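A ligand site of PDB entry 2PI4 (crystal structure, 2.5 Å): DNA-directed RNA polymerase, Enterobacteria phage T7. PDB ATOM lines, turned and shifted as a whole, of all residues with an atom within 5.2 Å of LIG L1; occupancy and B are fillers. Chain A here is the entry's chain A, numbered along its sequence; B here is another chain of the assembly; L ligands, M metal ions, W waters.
A nitrogen (N3) of LIG L1 sits close to an oxygen (O13) of LG2 L2, 3.4 Å away.
Residues that only touch LIG L1: Arg 420 (3.8 Å) and Arg 627 (3.7 Å).
Hydrophobic or aromatic side chains within 4 Å of LIG L1: Tyr 566, Tyr 634 and His 779.
Ten residues have an atom within 4 Å of LIG L1: Arg 420, Tyr 566, Arg 622, Lys 626, Arg 627, Tyr 634, His 779, Asp 807, DC 4 of chain B and DC 5 of chain B.
OD1 of Asp 807 sits at hydrogen-bond distance from O12 of LIG L1, at 2.6 Å.
N3 of DC 4 of chain B is in hydrogen-bond range of a nitrogen (N3) of LIG L1 (2.9 Å).
The side-chain hydroxyl of Tyr 566 lies within hydrogen-bond range of an oxygen (O5) of LIG L1 (2.9 Å).
A nitrogen (N5) of LIG L1 sits close to the side-chain hydroxyl of Tyr 634, 3.2 Å away.
A ring nitrogen (NE2) of His 779 lies within hydrogen-bond range of a nitrogen (N4) of LIG L1 (3.1 Å).
N4 of DC 5 of chain B is in hydrogen-bond range of N3 of LIG L1.
An oxygen (O3) of LIG L1 is in salt-bridge range of the guanidinium group of Arg 622 (3.5 Å).
NZ of Lys 626 is in salt-bridge range of O9 of LIG L1 (3.8 Å).
A nitrogen (N3) of LG2 L2 is in hydrogen-bond range of N3 of DC 5 of chain B (3.0 Å).
The side-chain carboxylate (OD2) of Asp 807 sits close to the side-chain carboxylate (OD1) of Asp 532, at 2.7 Å.
O2 of DC 4 of chain B sits at hydrogen-bond distance from NE2 of His 779 (3.2 Å).
OH of Tyr 566 sits at hydrogen-bond distance from SD of Met 630 (3.8 Å).
The guanidinium group (NH2) of Arg 420 lies close to a ring nitrogen (NE2) of His 779.
The guanidinium group of Arg 622 lies within salt-bridge range of the side-chain carboxylate of Asp 564, 3.2 Å away.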
ATOM      1  N   ARG A 420     -16.931 -15.915  32.052  1.00  0.00           N
ATOM      2  CA  ARG A 420     -16.477 -15.642  30.681  1.00  0.00           C
ATOM      3  C   ARG A 420     -16.917 -14.264  30.137  1.00  0.00           C
ATOM      4  O   ARG A 420     -18.058 -13.824  30.335  1.00  0.00           O
ATOM      5  CB  ARG A 420     -16.908 -16.774  29.722  1.00  0.00           C
ATOM      6  CG  ARG A 420     -16.092 -18.099  29.840  1.00  0.00           C
ATOM      7  CD  ARG A 420     -15.940 -18.796  28.461  1.00  0.00           C
ATOM      8  NE  ARG A 420     -15.129 -20.022  28.500  1.00  0.00           N
ATOM      9  CZ  ARG A 420     -15.042 -20.885  27.479  1.00  0.00           C
ATOM     10  NH1 ARG A 420     -15.702 -20.648  26.348  1.00  0.00           N
ATOM     11  NH2 ARG A 420     -14.335 -22.005  27.618  1.00  0.00           N
ATOM     12  N   ASP A 466      -0.381 -25.304  13.100  1.00  0.00           N
ATOM     13  CA  ASP A 466      -0.250 -25.177  14.547  1.00  0.00           C
ATOM     14  C   ASP A 466       0.253 -26.478  15.161  1.00  0.00           C
ATOM     15  O   ASP A 466       0.249 -26.654  16.377  1.00  0.00           O
ATOM     16  CB  ASP A 466      -1.605 -24.800  15.164  1.00  0.00           C
ATOM     17  CG  ASP A 466      -2.704 -24.629  14.106  1.00  0.00           C
ATOM     18  OD1 ASP A 466      -3.015 -25.609  13.385  1.00  0.00           O
ATOM     19  OD2 ASP A 466      -3.251 -23.512  14.009  1.00  0.00           O
ATOM     20  N   LYS A 467       0.691 -27.391  14.287  1.00  0.00           N
ATOM     21  CA  LYS A 467       1.204 -28.680  14.713  1.00  0.00           C
ATOM     22  C   LYS A 467       2.693 -28.819  14.376  1.00  0.00           C
ATOM     23  O   LYS A 467       3.072 -29.633  13.522  1.00  0.00           O
ATOM     24  CB  LYS A 467       0.381 -29.820  14.079  1.00  0.00           C
ATOM     25  CG  LYS A 467       0.124 -29.706  12.562  1.00  0.00           C
ATOM     26  CD  LYS A 467      -1.357 -29.509  12.243  1.00  0.00           C
ATOM     27  CE  LYS A 467      -2.211 -30.680  12.742  1.00  0.00           C
ATOM     28  NZ  LYS A 467      -3.675 -30.454  12.556  1.00  0.00           N
ATOM     29  N   ASP A 532      -3.997 -19.170  21.315  1.00  0.00           N
ATOM     30  CA  ASP A 532      -4.948 -20.131  21.834  1.00  0.00           C
ATOM     31  C   ASP A 532      -4.254 -21.429  22.321  1.00  0.00           C
ATOM     32  O   ASP A 532      -3.470 -22.036  21.581  1.00  0.00           O
ATOM     33  CB  ASP A 532      -5.987 -20.445  20.754  1.00  0.00           C
ATOM     34  CG  ASP A 532      -7.424 -20.473  21.297  1.00  0.00           C
ATOM     35  OD1 ASP A 532      -7.803 -19.509  22.013  1.00  0.00           O
ATOM     36  OD2 ASP A 532      -8.177 -21.438  20.989  1.00  0.00           O
ATOM     37  N   SER A 534      -4.059 -25.465  23.889  1.00  0.00           N
ATOM     38  CA  SER A 534      -4.286 -26.762  23.198  1.00  0.00           C
ATOM     39  C   SER A 534      -5.673 -27.331  23.512  1.00  0.00           C
ATOM     40  O   SER A 534      -6.304 -27.967  22.668  1.00  0.00           O
ATOM     41  CB  SER A 534      -3.199 -27.786  23.595  1.00  0.00           C
ATOM     42  OG  SER A 534      -3.286 -28.989  22.831  1.00  0.00           O
ATOM     43  N   SER A 536      -8.319 -25.830  26.490  1.00  0.00           N
ATOM     44  CA  SER A 536      -8.698 -25.132  27.704  1.00  0.00           C
ATOM     45  C   SER A 536      -9.441 -26.063  28.634  1.00  0.00           C
ATOM     46  O   SER A 536      -9.807 -27.181  28.266  1.00  0.00           O
ATOM     47  CB  SER A 536      -9.604 -23.921  27.402  1.00  0.00           C
ATOM     48  OG  SER A 536      -9.954 -23.200  28.576  1.00  0.00           O
ATOM     49  N   ASP A 564      -0.488 -33.234  20.292  1.00  0.00           N
ATOM     50  CA  ASP A 564      -1.872 -33.179  19.825  1.00  0.00           C
ATOM     51  C   ASP A 564      -2.723 -34.163  20.623  1.00  0.00           C
ATOM     52  O   ASP A 564      -2.875 -35.305  20.237  1.00  0.00           O
ATOM     53  CB  ASP A 564      -1.942 -33.536  18.328  1.00  0.00           C
ATOM     54  CG  ASP A 564      -3.315 -33.290  17.723  1.00  0.00           C
ATOM     55  OD1 ASP A 564      -3.785 -32.132  17.771  1.00  0.00           O
ATOM     56  OD2 ASP A 564      -3.914 -34.232  17.180  1.00  0.00           O
ATOM     57  N   TYR A 566      -5.669 -34.664  20.730  1.00  0.00           N
ATOM     58  CA  TYR A 566      -6.623 -35.394  19.911  1.00  0.00           C
ATOM     59  C   TYR A 566      -5.931 -36.522  19.175  1.00  0.00           C
ATOM     60  O   TYR A 566      -6.455 -37.625  19.080  1.00  0.00           O
ATOM     61  CB  TYR A 566      -7.293 -34.455  18.907  1.00  0.00           C
ATOM     62  CG  TYR A 566      -7.913 -33.234  19.537  1.00  0.00           C
ATOM     63  CD1 TYR A 566      -8.726 -33.356  20.664  1.00  0.00           C
ATOM     64  CD2 TYR A 566      -7.629 -31.959  19.047  1.00  0.00           C
ATOM     65  CE1 TYR A 566      -9.243 -32.229  21.312  1.00  0.00           C
ATOM     66  CE2 TYR A 566      -8.137 -30.818  19.688  1.00  0.00           C
ATOM     67  CZ  TYR A 566      -8.942 -30.957  20.823  1.00  0.00           C
ATOM     68  OH  TYR A 566      -9.405 -29.847  21.501  1.00  0.00           O
ATOM     69  N   ARG A 622      -6.973 -38.261  13.917  1.00  0.00           N
ATOM     70  CA  ARG A 622      -7.272 -37.266  14.951  1.00  0.00           C
ATOM     71  C   ARG A 622      -8.704 -36.801  14.775  1.00  0.00           C
ATOM     72  O   ARG A 622      -9.392 -36.417  15.729  1.00  0.00           O
ATOM     73  CB  ARG A 622      -6.304 -36.068  14.808  1.00  0.00           C
ATOM     74  CG  ARG A 622      -6.314 -35.381  13.407  1.00  0.00           C
ATOM     75  CD  ARG A 622      -5.075 -34.500  13.047  1.00  0.00           C
ATOM     76  NE  ARG A 622      -4.818 -33.383  13.964  1.00  0.00           N
ATOM     77  CZ  ARG A 622      -5.610 -32.324  14.169  1.00  0.00           C
ATOM     78  NH1 ARG A 622      -6.774 -32.193  13.538  1.00  0.00           N
ATOM     79  NH2 ARG A 622      -5.243 -31.378  15.027  1.00  0.00           N
ATOM     80  N   LYS A 626     -11.865 -36.381  17.993  1.00  0.00           N
ATOM     81  CA  LYS A 626     -11.732 -34.956  18.179  1.00  0.00           C
ATOM     82  C   LYS A 626     -12.768 -34.442  19.174  1.00  0.00           C
ATOM     83  O   LYS A 626     -12.509 -34.365  20.361  1.00  0.00           O
ATOM     84  CB  LYS A 626     -11.905 -34.237  16.838  1.00  0.00           C
ATOM     85  CG  LYS A 626     -11.253 -32.846  16.726  1.00  0.00           C
ATOM     86  CD  LYS A 626     -11.619 -31.903  17.871  1.00  0.00           C
ATOM     87  CE  LYS A 626     -11.387 -30.413  17.529  1.00  0.00           C
ATOM     88  NZ  LYS A 626     -12.275 -29.841  16.457  1.00  0.00           N
ATOM     89  N   ARG A 627     -13.935 -34.096  18.654  1.00  0.00           N
ATOM     90  CA  ARG A 627     -15.006 -33.544  19.465  1.00  0.00           C
ATOM     91  C   ARG A 627     -15.159 -34.271  20.780  1.00  0.00           C
ATOM     92  O   ARG A 627     -15.211 -33.654  21.834  1.00  0.00           O
ATOM     93  CB  ARG A 627     -16.314 -33.607  18.704  1.00  0.00           C
ATOM     94  CG  ARG A 627     -16.181 -33.185  17.267  1.00  0.00           C
ATOM     95  CD  ARG A 627     -17.146 -32.077  16.884  1.00  0.00           C
ATOM     96  NE  ARG A 627     -16.800 -30.776  17.453  1.00  0.00           N
ATOM     97  CZ  ARG A 627     -17.239 -30.333  18.632  1.00  0.00           C
ATOM     98  NH1 ARG A 627     -18.033 -31.086  19.383  1.00  0.00           N
ATOM     99  NH2 ARG A 627     -16.881 -29.118  19.037  1.00  0.00           N
ATOM    100  N   MET A 630     -12.659 -32.710  23.662  1.00  0.00           N
ATOM    101  CA  MET A 630     -12.907 -31.424  24.280  1.00  0.00           C
ATOM    102  C   MET A 630     -14.178 -31.503  25.092  1.00  0.00           C
ATOM    103  O   MET A 630     -14.229 -31.127  26.267  1.00  0.00           O
ATOM    104  CB  MET A 630     -13.052 -30.350  23.200  1.00  0.00           C
ATOM    105  CG  MET A 630     -13.858 -30.794  21.969  1.00  0.00           C
ATOM    106  SD  MET A 630     -12.945 -30.571  20.368  1.00  0.00           S
ATOM    107  CE  MET A 630     -13.821 -29.151  19.539  1.00  0.00           C
ATOM    108  N   TYR A 634     -17.140 -30.714  29.079  1.00  0.00           N
ATOM    109  CA  TYR A 634     -18.552 -30.351  29.243  1.00  0.00           C
ATOM    110  C   TYR A 634     -19.386 -31.480  29.787  1.00  0.00           C
ATOM    111  O   TYR A 634     -20.534 -31.285  30.192  1.00  0.00           O
ATOM    112  CB  TYR A 634     -19.164 -29.954  27.911  1.00  0.00           C
ATOM    113  CG  TYR A 634     -18.310 -29.013  27.154  1.00  0.00           C
ATOM    114  CD1 TYR A 634     -17.777 -27.896  27.793  1.00  0.00           C
ATOM    115  CD2 TYR A 634     -17.979 -29.249  25.828  1.00  0.00           C
ATOM    116  CE1 TYR A 634     -16.929 -27.039  27.131  1.00  0.00           C
ATOM    117  CE2 TYR A 634     -17.118 -28.392  25.151  1.00  0.00           C
ATOM    118  CZ  TYR A 634     -16.595 -27.293  25.820  1.00  0.00           C
ATOM    119  OH  TYR A 634     -15.680 -26.468  25.226  1.00  0.00           O
ATOM    120  N   HIS A 779     -15.010 -23.333  32.726  1.00  0.00           N
ATOM    121  CA  HIS A 779     -15.016 -22.048  32.059  1.00  0.00           C
ATOM    122  C   HIS A 779     -14.842 -21.026  33.150  1.00  0.00           C
ATOM    123  O   HIS A 779     -13.983 -20.142  33.035  1.00  0.00           O
ATOM    124  CB  HIS A 779     -16.336 -21.836  31.301  1.00  0.00           C
ATOM    125  CG  HIS A 779     -16.563 -22.796  30.168  1.00  0.00           C
ATOM    126  ND1 HIS A 779     -16.205 -24.124  30.241  1.00  0.00           N
ATOM    127  CD2 HIS A 779     -17.188 -22.635  28.985  1.00  0.00           C
ATOM    128  CE1 HIS A 779     -16.595 -24.745  29.143  1.00  0.00           C
ATOM    129  NE2 HIS A 779     -17.195 -23.869  28.364  1.00  0.00           N
ATOM    130  N   ASP A 807     -10.300 -17.657  25.523  1.00  0.00           N
ATOM    131  CA  ASP A 807      -9.039 -18.371  25.675  1.00  0.00           C
ATOM    132  C   ASP A 807      -8.062 -17.964  24.579  1.00  0.00           C
ATOM    133  O   ASP A 807      -6.978 -18.548  24.431  1.00  0.00           O
ATOM    134  CB  ASP A 807      -9.287 -19.873  25.571  1.00  0.00           C
ATOM    135  CG  ASP A 807      -9.900 -20.287  24.217  1.00  0.00           C
ATOM    136  OD1 ASP A 807     -10.163 -21.502  24.035  1.00  0.00           O
ATOM    137  OD2 ASP A 807     -10.109 -19.416  23.348  1.00  0.00           O
ATOM    138  P    DC B   4     -24.747 -30.612  28.372  1.00  0.00           P
ATOM    139  OP1  DC B   4     -25.039 -31.766  29.279  1.00  0.00           O
ATOM    140  OP2  DC B   4     -25.853 -29.939  27.682  1.00  0.00           O
ATOM    141  O5'  DC B   4     -24.024 -29.519  29.261  1.00  0.00           O
ATOM    142  C5'  DC B   4     -24.268 -28.190  28.983  1.00  0.00           C
ATOM    143  C4'  DC B   4     -23.387 -27.296  29.826  1.00  0.00           C
ATOM    144  O4'  DC B   4     -22.026 -27.450  29.355  1.00  0.00           O
ATOM    145  C3'  DC B   4     -23.756 -25.857  29.540  1.00  0.00           C
ATOM    146  O3'  DC B   4     -23.936 -25.032  30.652  1.00  0.00           O
ATOM    147  C2'  DC B   4     -22.845 -25.442  28.403  1.00  0.00           C
ATOM    148  C1'  DC B   4     -21.611 -26.308  28.577  1.00  0.00           C
ATOM    149  N1   DC B   4     -21.250 -26.807  27.252  1.00  0.00           N
ATOM    150  C2   DC B   4     -20.356 -26.080  26.453  1.00  0.00           C
ATOM    151  O2   DC B   4     -19.806 -25.068  26.906  1.00  0.00           O
ATOM    152  N3   DC B   4     -20.109 -26.517  25.192  1.00  0.00           N
ATOM    153  C4   DC B   4     -20.690 -27.628  24.748  1.00  0.00           C
ATOM    154  N4   DC B   4     -20.418 -28.042  23.509  1.00  0.00           N
ATOM    155  C5   DC B   4     -21.572 -28.393  25.555  1.00  0.00           C
ATOM    156  C6   DC B   4     -21.817 -27.953  26.792  1.00  0.00           C
ATOM    157  P    DC B   5     -25.276 -24.168  30.728  1.00  0.00           P
ATOM    158  OP1  DC B   5     -25.976 -24.511  31.993  1.00  0.00           O
ATOM    159  OP2  DC B   5     -25.972 -24.355  29.418  1.00  0.00           O
ATOM    160  O5'  DC B   5     -24.707 -22.691  30.787  1.00  0.00           O
ATOM    161  C5'  DC B   5     -23.452 -22.428  30.205  1.00  0.00           C
ATOM    162  C4'  DC B   5     -23.382 -21.010  29.699  1.00  0.00           C
ATOM    163  O4'  DC B   5     -22.482 -21.035  28.571  1.00  0.00           O
ATOM    164  C3'  DC B   5     -24.720 -20.516  29.146  1.00  0.00           C
ATOM    165  O3'  DC B   5     -24.859 -19.097  29.300  1.00  0.00           O
ATOM    166  C2'  DC B   5     -24.676 -20.960  27.701  1.00  0.00           C
ATOM    167  C1'  DC B   5     -23.193 -20.868  27.369  1.00  0.00           C
ATOM    168  N1   DC B   5     -22.742 -21.901  26.423  1.00  0.00           N
ATOM    169  C2   DC B   5     -21.596 -21.666  25.683  1.00  0.00           C
ATOM    170  O2   DC B   5     -20.930 -20.644  25.920  1.00  0.00           O
ATOM    171  N3   DC B   5     -21.231 -22.552  24.736  1.00  0.00           N
ATOM    172  C4   DC B   5     -21.957 -23.651  24.537  1.00  0.00           C
ATOM    173  N4   DC B   5     -21.589 -24.484  23.569  1.00  0.00           N
ATOM    174  C5   DC B   5     -23.118 -23.940  25.314  1.00  0.00           C
ATOM    175  C6   DC B   5     -23.469 -23.040  26.247  1.00  0.00           C
HETATM  176  P1  LIG L   1      -7.310 -27.620  15.899  1.00  0.00           P
HETATM  177  O1  LIG L   1      -8.108 -28.643  15.133  1.00  0.00           O
HETATM  178  O2  LIG L   1      -7.422 -26.165  15.489  1.00  0.00           O
HETATM  179  O3  LIG L   1      -5.771 -28.004  15.723  1.00  0.00           O
HETATM  180  O4  LIG L   1      -7.595 -27.845  17.543  1.00  0.00           O
HETATM  181  P2  LIG L   1      -8.671 -26.943  18.326  1.00  0.00           P
HETATM  182  O5  LIG L   1      -8.933 -27.713  19.535  1.00  0.00           O
HETATM  183  O6  LIG L   1      -8.154 -25.582  18.583  1.00  0.00           O
HETATM  184  O7  LIG L   1     -10.036 -26.880  17.444  1.00  0.00           O
HETATM  185  P3  LIG L   1     -11.061 -25.625  16.939  1.00  0.00           P
HETATM  186  O8  LIG L   1     -10.274 -24.580  16.169  1.00  0.00           O
HETATM  187  O9  LIG L   1     -12.417 -26.053  16.502  1.00  0.00           O
HETATM  188  O10 LIG L   1     -11.344 -24.925  18.352  1.00  0.00           O
HETATM  189  C1  LIG L   1     -12.176 -23.797  18.513  1.00  0.00           C
HETATM  190  C2  LIG L   1     -12.245 -23.360  19.975  1.00  0.00           C
HETATM  191  O11 LIG L   1     -13.500 -22.735  20.387  1.00  0.00           O
HETATM  192  C3  LIG L   1     -11.914 -24.503  20.934  1.00  0.00           C
HETATM  193  C4  LIG L   1     -12.672 -24.066  22.225  1.00  0.00           C
HETATM  194  O12 LIG L   1     -11.879 -23.308  23.236  1.00  0.00           O
HETATM  195  C5  LIG L   1     -13.897 -23.307  21.635  1.00  0.00           C
HETATM  196  N1  LIG L   1     -15.019 -24.187  21.348  1.00  0.00           N
HETATM  197  C6  LIG L   1     -15.303 -24.975  20.266  1.00  0.00           C
HETATM  198  N2  LIG L   1     -16.397 -25.671  20.324  1.00  0.00           N
HETATM  199  C7  LIG L   1     -16.887 -25.316  21.561  1.00  0.00           C
HETATM  200  C8  LIG L   1     -18.058 -25.734  22.245  1.00  0.00           C
HETATM  201  O13 LIG L   1     -18.898 -26.512  21.859  1.00  0.00           O
HETATM  202  N3  LIG L   1     -18.226 -25.133  23.501  1.00  0.00           N
HETATM  203  C9  LIG L   1     -17.328 -24.209  24.073  1.00  0.00           C
HETATM  204  N4  LIG L   1     -17.605 -23.706  25.298  1.00  0.00           N
HETATM  205  N5  LIG L   1     -16.203 -23.813  23.427  1.00  0.00           N
HETATM  206  C10 LIG L   1     -16.046 -24.401  22.188  1.00  0.00           C
HETATM  207  P1  LG2 L   2     -18.708 -21.260  10.834  1.00  0.00           P
HETATM  208  O1  LG2 L   2     -19.816 -20.254  10.627  1.00  0.00           O
HETATM  209  O2  LG2 L   2     -18.873 -22.626  10.219  1.00  0.00           O
HETATM  210  O3  LG2 L   2     -17.387 -20.638  10.153  1.00  0.00           O
HETATM  211  O4  LG2 L   2     -18.377 -21.361  12.491  1.00  0.00           O
HETATM  212  P2  LG2 L   2     -17.927 -20.076  13.382  1.00  0.00           P
HETATM  213  O5  LG2 L   2     -16.550 -20.413  13.764  1.00  0.00           O
HETATM  214  O6  LG2 L   2     -18.048 -18.835  12.615  1.00  0.00           O
HETATM  215  O7  LG2 L   2     -18.849 -19.962  14.754  1.00  0.00           O
HETATM  216  P3  LG2 L   2     -19.320 -18.642  15.775  1.00  0.00           P
HETATM  217  O8  LG2 L   2     -19.248 -17.334  15.031  1.00  0.00           O
HETATM  218  O9  LG2 L   2     -20.455 -18.913  16.705  1.00  0.00           O
HETATM  219  O10 LG2 L   2     -18.082 -18.612  16.814  1.00  0.00           O
HETATM  220  C1  LG2 L   2     -16.813 -17.979  16.548  1.00  0.00           C
HETATM  221  C2  LG2 L   2     -15.901 -18.169  17.749  1.00  0.00           C
HETATM  222  O11 LG2 L   2     -16.526 -18.345  19.084  1.00  0.00           O
HETATM  223  C3  LG2 L   2     -14.921 -19.294  17.490  1.00  0.00           C
HETATM  224  C4  LG2 L   2     -14.547 -19.719  18.921  1.00  0.00           C
HETATM  225  O12 LG2 L   2     -13.398 -18.976  19.486  1.00  0.00           O
HETATM  226  C5  LG2 L   2     -15.852 -19.447  19.719  1.00  0.00           C
HETATM  227  N1  LG2 L   2     -16.843 -20.539  19.741  1.00  0.00           N
HETATM  228  C6  LG2 L   2     -17.224 -21.457  18.795  1.00  0.00           C
HETATM  229  N2  LG2 L   2     -18.160 -22.308  19.148  1.00  0.00           N
HETATM  230  C7  LG2 L   2     -18.431 -21.889  20.454  1.00  0.00           C
HETATM  231  C8  LG2 L   2     -19.360 -22.387  21.442  1.00  0.00           C
HETATM  232  O13 LG2 L   2     -20.150 -23.294  21.354  1.00  0.00           O
HETATM  233  N3  LG2 L   2     -19.325 -21.696  22.650  1.00  0.00           N
HETATM  234  C9  LG2 L   2     -18.480 -20.622  22.923  1.00  0.00           C
HETATM  235  N4  LG2 L   2     -18.570 -20.037  24.126  1.00  0.00           N
HETATM  236  N5  LG2 L   2     -17.606 -20.143  22.018  1.00  0.00           N
HETATM  237  C10 LG2 L   2     -17.626 -20.815  20.810  1.00  0.00           C
HETATM  238 MG    MG M   1      -8.909 -23.173  21.110  1.00  0.00          MG
HETATM  239  O   HOH W   1     -13.222 -26.799  13.287  1.00  0.00           O
